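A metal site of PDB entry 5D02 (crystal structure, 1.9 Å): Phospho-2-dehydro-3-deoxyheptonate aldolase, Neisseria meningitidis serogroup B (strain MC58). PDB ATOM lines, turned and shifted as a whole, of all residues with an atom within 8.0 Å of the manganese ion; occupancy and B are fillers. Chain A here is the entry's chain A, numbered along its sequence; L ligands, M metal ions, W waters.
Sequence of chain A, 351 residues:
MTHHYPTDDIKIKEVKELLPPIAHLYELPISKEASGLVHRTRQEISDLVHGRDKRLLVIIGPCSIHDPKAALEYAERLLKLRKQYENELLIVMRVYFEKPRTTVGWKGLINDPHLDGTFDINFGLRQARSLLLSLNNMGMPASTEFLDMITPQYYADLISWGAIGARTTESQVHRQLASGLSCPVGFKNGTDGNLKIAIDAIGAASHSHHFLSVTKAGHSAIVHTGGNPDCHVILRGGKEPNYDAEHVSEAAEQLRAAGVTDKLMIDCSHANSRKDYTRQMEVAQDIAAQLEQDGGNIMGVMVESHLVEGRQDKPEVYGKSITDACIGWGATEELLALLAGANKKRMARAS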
ATOM      1  N   GLY A  61     -21.256 -13.575 -23.724  1.00  0.00           N
ATOM      2  CA  GLY A  61     -22.164 -12.442 -23.979  1.00  0.00           C
ATOM      3  C   GLY A  61     -21.537 -11.430 -24.926  1.00  0.00           C
ATOM      4  O   GLY A  61     -20.556 -11.740 -25.579  1.00  0.00           O
ATOM      5  N   PRO A  62     -22.130 -10.238 -25.022  1.00  0.00           N
ATOM      6  CA  PRO A  62     -21.775  -9.289 -26.062  1.00  0.00           C
ATOM      7  C   PRO A  62     -20.304  -8.851 -25.965  1.00  0.00           C
ATOM      8  O   PRO A  62     -19.728  -8.877 -24.880  1.00  0.00           O
ATOM      9  CB  PRO A  62     -22.714  -8.117 -25.779  1.00  0.00           C
ATOM     10  CG  PRO A  62     -23.920  -8.764 -25.176  1.00  0.00           C
ATOM     11  CD  PRO A  62     -23.360  -9.854 -24.301  1.00  0.00           C
ATOM     12  N   CYS A  63     -19.706  -8.524 -27.109  1.00  0.00           N
ATOM     13  CA  CYS A  63     -18.420  -7.896 -27.134  1.00  0.00           C
ATOM     14  C   CYS A  63     -18.451  -6.665 -26.221  1.00  0.00           C
ATOM     15  O   CYS A  63     -17.581  -6.469 -25.366  1.00  0.00           O
ATOM     16  CB  CYS A  63     -18.048  -7.479 -28.570  1.00  0.00           C
ATOM     17  SG  CYS A  63     -16.484  -6.516 -28.632  1.00  0.00           S
ATOM     18  N   SER A  64     -19.492  -5.843 -26.398  1.00  0.00           N
ATOM     19  CA  SER A  64     -19.724  -4.655 -25.596  1.00  0.00           C
ATOM     20  C   SER A  64     -21.234  -4.433 -25.295  1.00  0.00           C
ATOM     21  O   SER A  64     -22.090  -4.794 -26.106  1.00  0.00           O
ATOM     22  CB  SER A  64     -19.188  -3.428 -26.306  1.00  0.00           C
ATOM     23  OG  SER A  64     -19.840  -3.172 -27.536  1.00  0.00           O
ATOM     24  N   ARG A  94     -20.856 -11.906 -19.942  1.00  0.00           N
ATOM     25  CA  ARG A  94     -19.967 -10.820 -20.350  1.00  0.00           C
ATOM     26  C   ARG A  94     -20.753  -9.525 -20.306  1.00  0.00           C
ATOM     27  O   ARG A  94     -21.725  -9.360 -21.080  1.00  0.00           O
ATOM     28  CB  ARG A  94     -19.528 -10.983 -21.826  1.00  0.00           C
ATOM     29  CG  ARG A  94     -18.288 -11.759 -22.065  1.00  0.00           C
ATOM     30  CD  ARG A  94     -17.825 -11.730 -23.535  1.00  0.00           C
ATOM     31  NE  ARG A  94     -17.419 -10.428 -24.060  1.00  0.00           N
ATOM     32  CZ  ARG A  94     -16.157 -10.037 -24.289  1.00  0.00           C
ATOM     33  NH1 ARG A  94     -15.122 -10.853 -24.082  1.00  0.00           N
ATOM     34  NH2 ARG A  94     -15.914  -8.823 -24.764  1.00  0.00           N
ATOM     35  N   TYR A  96     -19.332  -6.014 -20.632  1.00  0.00           N
ATOM     36  CA  TYR A  96     -18.152  -5.169 -20.849  1.00  0.00           C
ATOM     37  C   TYR A  96     -18.579  -3.737 -21.190  1.00  0.00           C
ATOM     38  O   TYR A  96     -19.240  -3.514 -22.181  1.00  0.00           O
ATOM     39  CB  TYR A  96     -17.278  -5.728 -21.951  1.00  0.00           C
ATOM     40  CG  TYR A  96     -16.393  -6.911 -21.542  1.00  0.00           C
ATOM     41  CD1 TYR A  96     -16.882  -7.957 -20.754  1.00  0.00           C
ATOM     42  CD2 TYR A  96     -15.094  -7.001 -21.976  1.00  0.00           C
ATOM     43  CE1 TYR A  96     -16.071  -9.020 -20.392  1.00  0.00           C
ATOM     44  CE2 TYR A  96     -14.289  -8.094 -21.658  1.00  0.00           C
ATOM     45  CZ  TYR A  96     -14.789  -9.101 -20.867  1.00  0.00           C
ATOM     46  OH  TYR A  96     -14.006 -10.160 -20.528  1.00  0.00           O
ATOM     47  N   LYS A  99     -13.902  -0.575 -23.386  1.00  0.00           N
ATOM     48  CA  LYS A  99     -13.346  -1.154 -24.622  1.00  0.00           C
ATOM     49  C   LYS A  99     -12.048  -0.471 -25.005  1.00  0.00           C
ATOM     50  O   LYS A  99     -12.000   0.767 -25.146  1.00  0.00           O
ATOM     51  CB  LYS A  99     -14.334  -1.000 -25.806  1.00  0.00           C
ATOM     52  CG  LYS A  99     -15.662  -1.607 -25.549  1.00  0.00           C
ATOM     53  CD  LYS A  99     -15.545  -3.042 -25.025  1.00  0.00           C
ATOM     54  CE  LYS A  99     -15.106  -4.025 -26.141  1.00  0.00           C
ATOM     55  NZ  LYS A  99     -14.926  -5.353 -25.586  1.00  0.00           N
ATOM     56  N   PRO A 100     -10.994  -1.266 -25.219  1.00  0.00           N
ATOM     57  CA  PRO A 100      -9.704  -0.707 -25.628  1.00  0.00           C
ATOM     58  C   PRO A 100      -9.657  -0.648 -27.148  1.00  0.00           C
ATOM     59  O   PRO A 100      -9.878  -1.656 -27.803  1.00  0.00           O
ATOM     60  CB  PRO A 100      -8.694  -1.713 -25.091  1.00  0.00           C
ATOM     61  CG  PRO A 100      -9.426  -3.005 -24.962  1.00  0.00           C
ATOM     62  CD  PRO A 100     -10.912  -2.694 -24.881  1.00  0.00           C
ATOM     63  N   GLU A 145     -14.214  -6.319 -18.292  1.00  0.00           N
ATOM     64  CA  GLU A 145     -12.788  -6.001 -18.387  1.00  0.00           C
ATOM     65  C   GLU A 145     -12.583  -4.706 -17.618  1.00  0.00           C
ATOM     66  O   GLU A 145     -13.278  -3.714 -17.883  1.00  0.00           O
ATOM     67  CB  GLU A 145     -12.279  -5.796 -19.831  1.00  0.00           C
ATOM     68  CG  GLU A 145     -10.777  -5.389 -19.885  1.00  0.00           C
ATOM     69  CD  GLU A 145     -10.207  -4.966 -21.265  1.00  0.00           C
ATOM     70  OE1 GLU A 145     -10.732  -5.388 -22.305  1.00  0.00           O
ATOM     71  OE2 GLU A 145      -9.205  -4.193 -21.299  1.00  0.00           O
ATOM     72  N   ARG A 167      -3.965  -5.736 -24.236  1.00  0.00           N
ATOM     73  CA  ARG A 167      -3.201  -4.506 -24.409  1.00  0.00           C
ATOM     74  C   ARG A 167      -2.700  -3.918 -23.078  1.00  0.00           C
ATOM     75  O   ARG A 167      -1.979  -2.922 -23.071  1.00  0.00           O
ATOM     76  CB  ARG A 167      -4.053  -3.462 -25.145  1.00  0.00           C
ATOM     77  CG  ARG A 167      -4.341  -3.924 -26.566  1.00  0.00           C
ATOM     78  CD  ARG A 167      -5.340  -3.073 -27.323  1.00  0.00           C
ATOM     79  NE  ARG A 167      -5.716  -3.748 -28.578  1.00  0.00           N
ATOM     80  CZ  ARG A 167      -6.564  -4.789 -28.698  1.00  0.00           C
ATOM     81  NH1 ARG A 167      -7.169  -5.369 -27.646  1.00  0.00           N
ATOM     82  NH2 ARG A 167      -6.804  -5.288 -29.904  1.00  0.00           N
ATOM     83  N   LYS A 188      -5.166 -11.814 -20.259  1.00  0.00           N
ATOM     84  CA  LYS A 188      -5.038 -12.265 -21.626  1.00  0.00           C
ATOM     85  C   LYS A 188      -3.597 -12.232 -22.099  1.00  0.00           C
ATOM     86  O   LYS A 188      -2.854 -11.320 -21.764  1.00  0.00           O
ATOM     87  CB  LYS A 188      -5.888 -11.385 -22.513  1.00  0.00           C
ATOM     88  CG  LYS A 188      -7.361 -11.674 -22.298  1.00  0.00           C
ATOM     89  CD  LYS A 188      -8.240 -11.077 -23.354  1.00  0.00           C
ATOM     90  CE  LYS A 188      -9.333 -12.079 -23.704  1.00  0.00           C
ATOM     91  NZ  LYS A 188     -10.073 -11.551 -24.872  1.00  0.00           N
ATOM     92  N   ASP A 267     -10.241 -18.260 -25.030  1.00  0.00           N
ATOM     93  CA  ASP A 267     -11.171 -17.356 -25.711  1.00  0.00           C
ATOM     94  C   ASP A 267     -11.394 -17.927 -27.107  1.00  0.00           C
ATOM     95  O   ASP A 267     -10.450 -18.169 -27.827  1.00  0.00           O
ATOM     96  CB  ASP A 267     -10.560 -15.928 -25.748  1.00  0.00           C
ATOM     97  CG  ASP A 267     -11.484 -14.858 -26.399  1.00  0.00           C
ATOM     98  OD1 ASP A 267     -12.627 -15.170 -26.855  1.00  0.00           O
ATOM     99  OD2 ASP A 267     -11.021 -13.677 -26.433  1.00  0.00           O
ATOM    100  N   SER A 269     -13.010 -16.266 -29.399  1.00  0.00           N
ATOM    101  CA  SER A 269     -13.153 -15.116 -30.306  1.00  0.00           C
ATOM    102  C   SER A 269     -11.811 -14.408 -30.477  1.00  0.00           C
ATOM    103  O   SER A 269     -10.742 -15.034 -30.324  1.00  0.00           O
ATOM    104  CB  SER A 269     -14.242 -14.170 -29.774  1.00  0.00           C
ATOM    105  OG  SER A 269     -14.764 -13.289 -30.761  1.00  0.00           O
ATOM    106  N   HIS A 270     -11.848 -13.130 -30.868  1.00  0.00           N
ATOM    107  CA  HIS A 270     -10.661 -12.314 -31.087  1.00  0.00           C
ATOM    108  C   HIS A 270      -9.657 -13.022 -31.987  1.00  0.00           C
ATOM    109  O   HIS A 270     -10.024 -13.473 -33.052  1.00  0.00           O
ATOM    110  CB  HIS A 270     -10.118 -11.819 -29.751  1.00  0.00           C
ATOM    111  CG  HIS A 270     -11.163 -11.122 -28.969  1.00  0.00           C
ATOM    112  ND1 HIS A 270     -11.811 -11.704 -27.903  1.00  0.00           N
ATOM    113  CD2 HIS A 270     -11.777  -9.936 -29.191  1.00  0.00           C
ATOM    114  CE1 HIS A 270     -12.764 -10.900 -27.482  1.00  0.00           C
ATOM    115  NE2 HIS A 270     -12.750  -9.804 -28.243  1.00  0.00           N
ATOM    116  N   MET A 302     -14.275 -18.443 -23.200  1.00  0.00           N
ATOM    117  CA  MET A 302     -14.835 -17.111 -23.398  1.00  0.00           C
ATOM    118  C   MET A 302     -15.467 -17.096 -24.776  1.00  0.00           C
ATOM    119  O   MET A 302     -14.907 -17.667 -25.716  1.00  0.00           O
ATOM    120  CB  MET A 302     -13.775 -16.017 -23.245  1.00  0.00           C
ATOM    121  CG  MET A 302     -14.280 -14.617 -23.569  1.00  0.00           C
ATOM    122  SD  MET A 302     -13.017 -13.326 -23.295  1.00  0.00           S
ATOM    123  CE  MET A 302     -12.929 -13.259 -21.500  1.00  0.00           C
ATOM    124  N   GLU A 304     -18.017 -14.600 -27.544  1.00  0.00           N
ATOM    125  CA  GLU A 304     -18.670 -13.358 -27.937  1.00  0.00           C
ATOM    126  C   GLU A 304     -20.004 -13.667 -28.641  1.00  0.00           C
ATOM    127  O   GLU A 304     -20.029 -14.146 -29.787  1.00  0.00           O
ATOM    128  CB  GLU A 304     -17.726 -12.510 -28.782  1.00  0.00           C
ATOM    129  CG  GLU A 304     -16.674 -11.831 -27.928  1.00  0.00           C
ATOM    130  CD  GLU A 304     -15.917 -10.732 -28.645  1.00  0.00           C
ATOM    131  OE1 GLU A 304     -15.399 -10.990 -29.746  1.00  0.00           O
ATOM    132  OE2 GLU A 304     -15.801  -9.632 -28.063  1.00  0.00           O
ATOM    133  N   SER A 321     -24.305  -6.311 -32.121  1.00  0.00           N
ATOM    134  CA  SER A 321     -23.072  -5.649 -31.723  1.00  0.00           C
ATOM    135  C   SER A 321     -22.730  -4.459 -32.594  1.00  0.00           C
ATOM    136  O   SER A 321     -22.871  -4.517 -33.796  1.00  0.00           O
ATOM    137  CB  SER A 321     -21.885  -6.620 -31.778  1.00  0.00           C
ATOM    138  OG  SER A 321     -20.685  -6.000 -31.237  1.00  0.00           O
ATOM    139  N   THR A 323     -19.513  -3.372 -31.832  1.00  0.00           N
ATOM    140  CA  THR A 323     -18.048  -3.553 -31.789  1.00  0.00           C
ATOM    141  C   THR A 323     -17.743  -4.875 -32.506  1.00  0.00           C
ATOM    142  O   THR A 323     -18.152  -5.029 -33.642  1.00  0.00           O
ATOM    143  CB  THR A 323     -17.498  -3.439 -30.355  1.00  0.00           C
ATOM    144  OG1 THR A 323     -18.247  -4.273 -29.443  1.00  0.00           O
ATOM    145  CG2 THR A 323     -17.594  -1.988 -29.911  1.00  0.00           C
ATOM    146  N   ASP A 324     -17.098  -5.848 -31.889  1.00  0.00           N
ATOM    147  CA  ASP A 324     -16.786  -7.091 -32.647  1.00  0.00           C
ATOM    148  C   ASP A 324     -18.056  -7.904 -32.966  1.00  0.00           C
ATOM    149  O   ASP A 324     -19.034  -7.869 -32.234  1.00  0.00           O
ATOM    150  CB  ASP A 324     -15.822  -8.002 -31.902  1.00  0.00           C
ATOM    151  CG  ASP A 324     -14.489  -7.336 -31.622  1.00  0.00           C
ATOM    152  OD1 ASP A 324     -14.028  -6.516 -32.400  1.00  0.00           O
ATOM    153  OD2 ASP A 324     -13.921  -7.639 -30.581  1.00  0.00           O
ATOM    154  N   ALA A 325     -18.015  -8.627 -34.082  1.00  0.00           N
ATOM    155  CA  ALA A 325     -19.114  -9.480 -34.496  1.00  0.00           C
ATOM    156  C   ALA A 325     -19.285 -10.654 -33.540  1.00  0.00           C
ATOM    157  O   ALA A 325     -18.315 -11.209 -33.067  1.00  0.00           O
ATOM    158  CB  ALA A 325     -18.922  -9.971 -35.941  1.00  0.00           C
ATOM    159  N   CYS A 326     -20.545 -10.961 -33.199  1.00  0.00           N
ATOM    160  CA  CYS A 326     -20.864 -11.997 -32.246  1.00  0.00           C
ATOM    161  C   CYS A 326     -21.686 -13.087 -32.927  1.00  0.00           C
ATOM    162  O   CYS A 326     -22.342 -12.818 -33.953  1.00  0.00           O
ATOM    163  CB  CYS A 326     -21.702 -11.401 -31.105  1.00  0.00           C
ATOM    164  SG  CYS A 326     -20.803 -10.205 -30.087  1.00  0.00           S
HETATM  165  C1  LIG L   1     -12.455  -8.441 -25.100  1.00  0.00           C
HETATM  166  O1  LIG L   1     -12.407  -9.528 -24.482  1.00  0.00           O
HETATM  167  O2  LIG L   1     -13.471  -7.879 -25.558  1.00  0.00           O
HETATM  168  C2  LIG L   1     -11.218  -7.857 -25.472  1.00  0.00           C
HETATM  169  C3  LIG L   1     -11.051  -6.529 -25.578  1.00  0.00           C
HETATM  170  O3  LIG L   1     -10.259  -8.841 -25.843  1.00  0.00           O
HETATM  171  P1  LIG L   1      -8.646  -8.583 -26.104  1.00  0.00           P
HETATM  172  O4  LIG L   1      -8.053  -7.826 -24.903  1.00  0.00           O
HETATM  173  O5  LIG L   1      -8.284 -10.054 -26.355  1.00  0.00           O
HETATM  174  O6  LIG L   1      -8.605  -7.810 -27.388  1.00  0.00           O
HETATM  175 MN    MN M   1     -14.460  -8.159 -28.580  1.00  0.00          MN
HETATM  176  O   HOH W   1     -13.425  -6.483 -27.793  1.00  0.00           O
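The side-chain hydroxyl (OG1) of Thr 323 sits close to the side-chain sulfur (SG) of Cys 63, 3.0 Å away.
The side-chain amino group of Lys 188 lies within hydrogen-bond range of a ring nitrogen (ND1) of His 270 (3.5 Å).
The guanidinium group (NH2) of Arg 94 lies within hydrogen-bond range of the backbone carbonyl oxygen (O) of Cys 63 (2.9 Å).
The side-chain sulfur (SG) of Cys 326 is in hydrogen-bond range of the backbone carbonyl oxygen (O) of Asp 324.
NZ of Lys 99 sits at hydrogen-bond distance from O of Cys 63 (2.9 Å).
The side-chain carboxylate of Asp 267 lies within hydrogen-bond range of a ring nitrogen (ND1) of His 270 (2.6 Å).
NH2 of Arg 94 sits close to OE2 of Glu 304, at 3.4 Å.
The side-chain carboxylate (OE1) of Glu 304 is in hydrogen-bond range of the side-chain hydroxyl (OG) of Ser 269.
The guanidinium group (NH2) of Arg 94 lies within salt-bridge range of an oxygen (O2) of the ligand, at 2.7 Å.
A ring nitrogen (NE2) of His 270 lies close to an oxygen (O2) of the ligand.
An oxygen (O2) of the ligand lies within salt-bridge range of the side-chain amino group of Lys 99, 2.9 Å away.
NH1 of Arg 167 lies within salt-bridge range of O6 of the ligand, 2.8 Å away.
NZ of Lys 188 is in salt-bridge range of O5 of the ligand (2.8 Å).
Four residues have an atom within 4 Å of the manganese ion: Cys 63, His 270, Glu 304 and Asp 324.
The nearest printed residue that does not touch the manganese ion is Lys 99 (4.1 Å).
The manganese ion is bound by OE2 of Glu 304 (2.1 Å), water W1 (2.1 Å), OD2 of Asp 324 (2.1 Å), NE2 of His 270 (2.4 Å) and SG of Cys 63 (2.6 Å).
The manganese ion has five donor atoms within binding distance.
Water W1 lies within hydrogen-bond range of O2 of the ligand and NZ of Lys 99.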
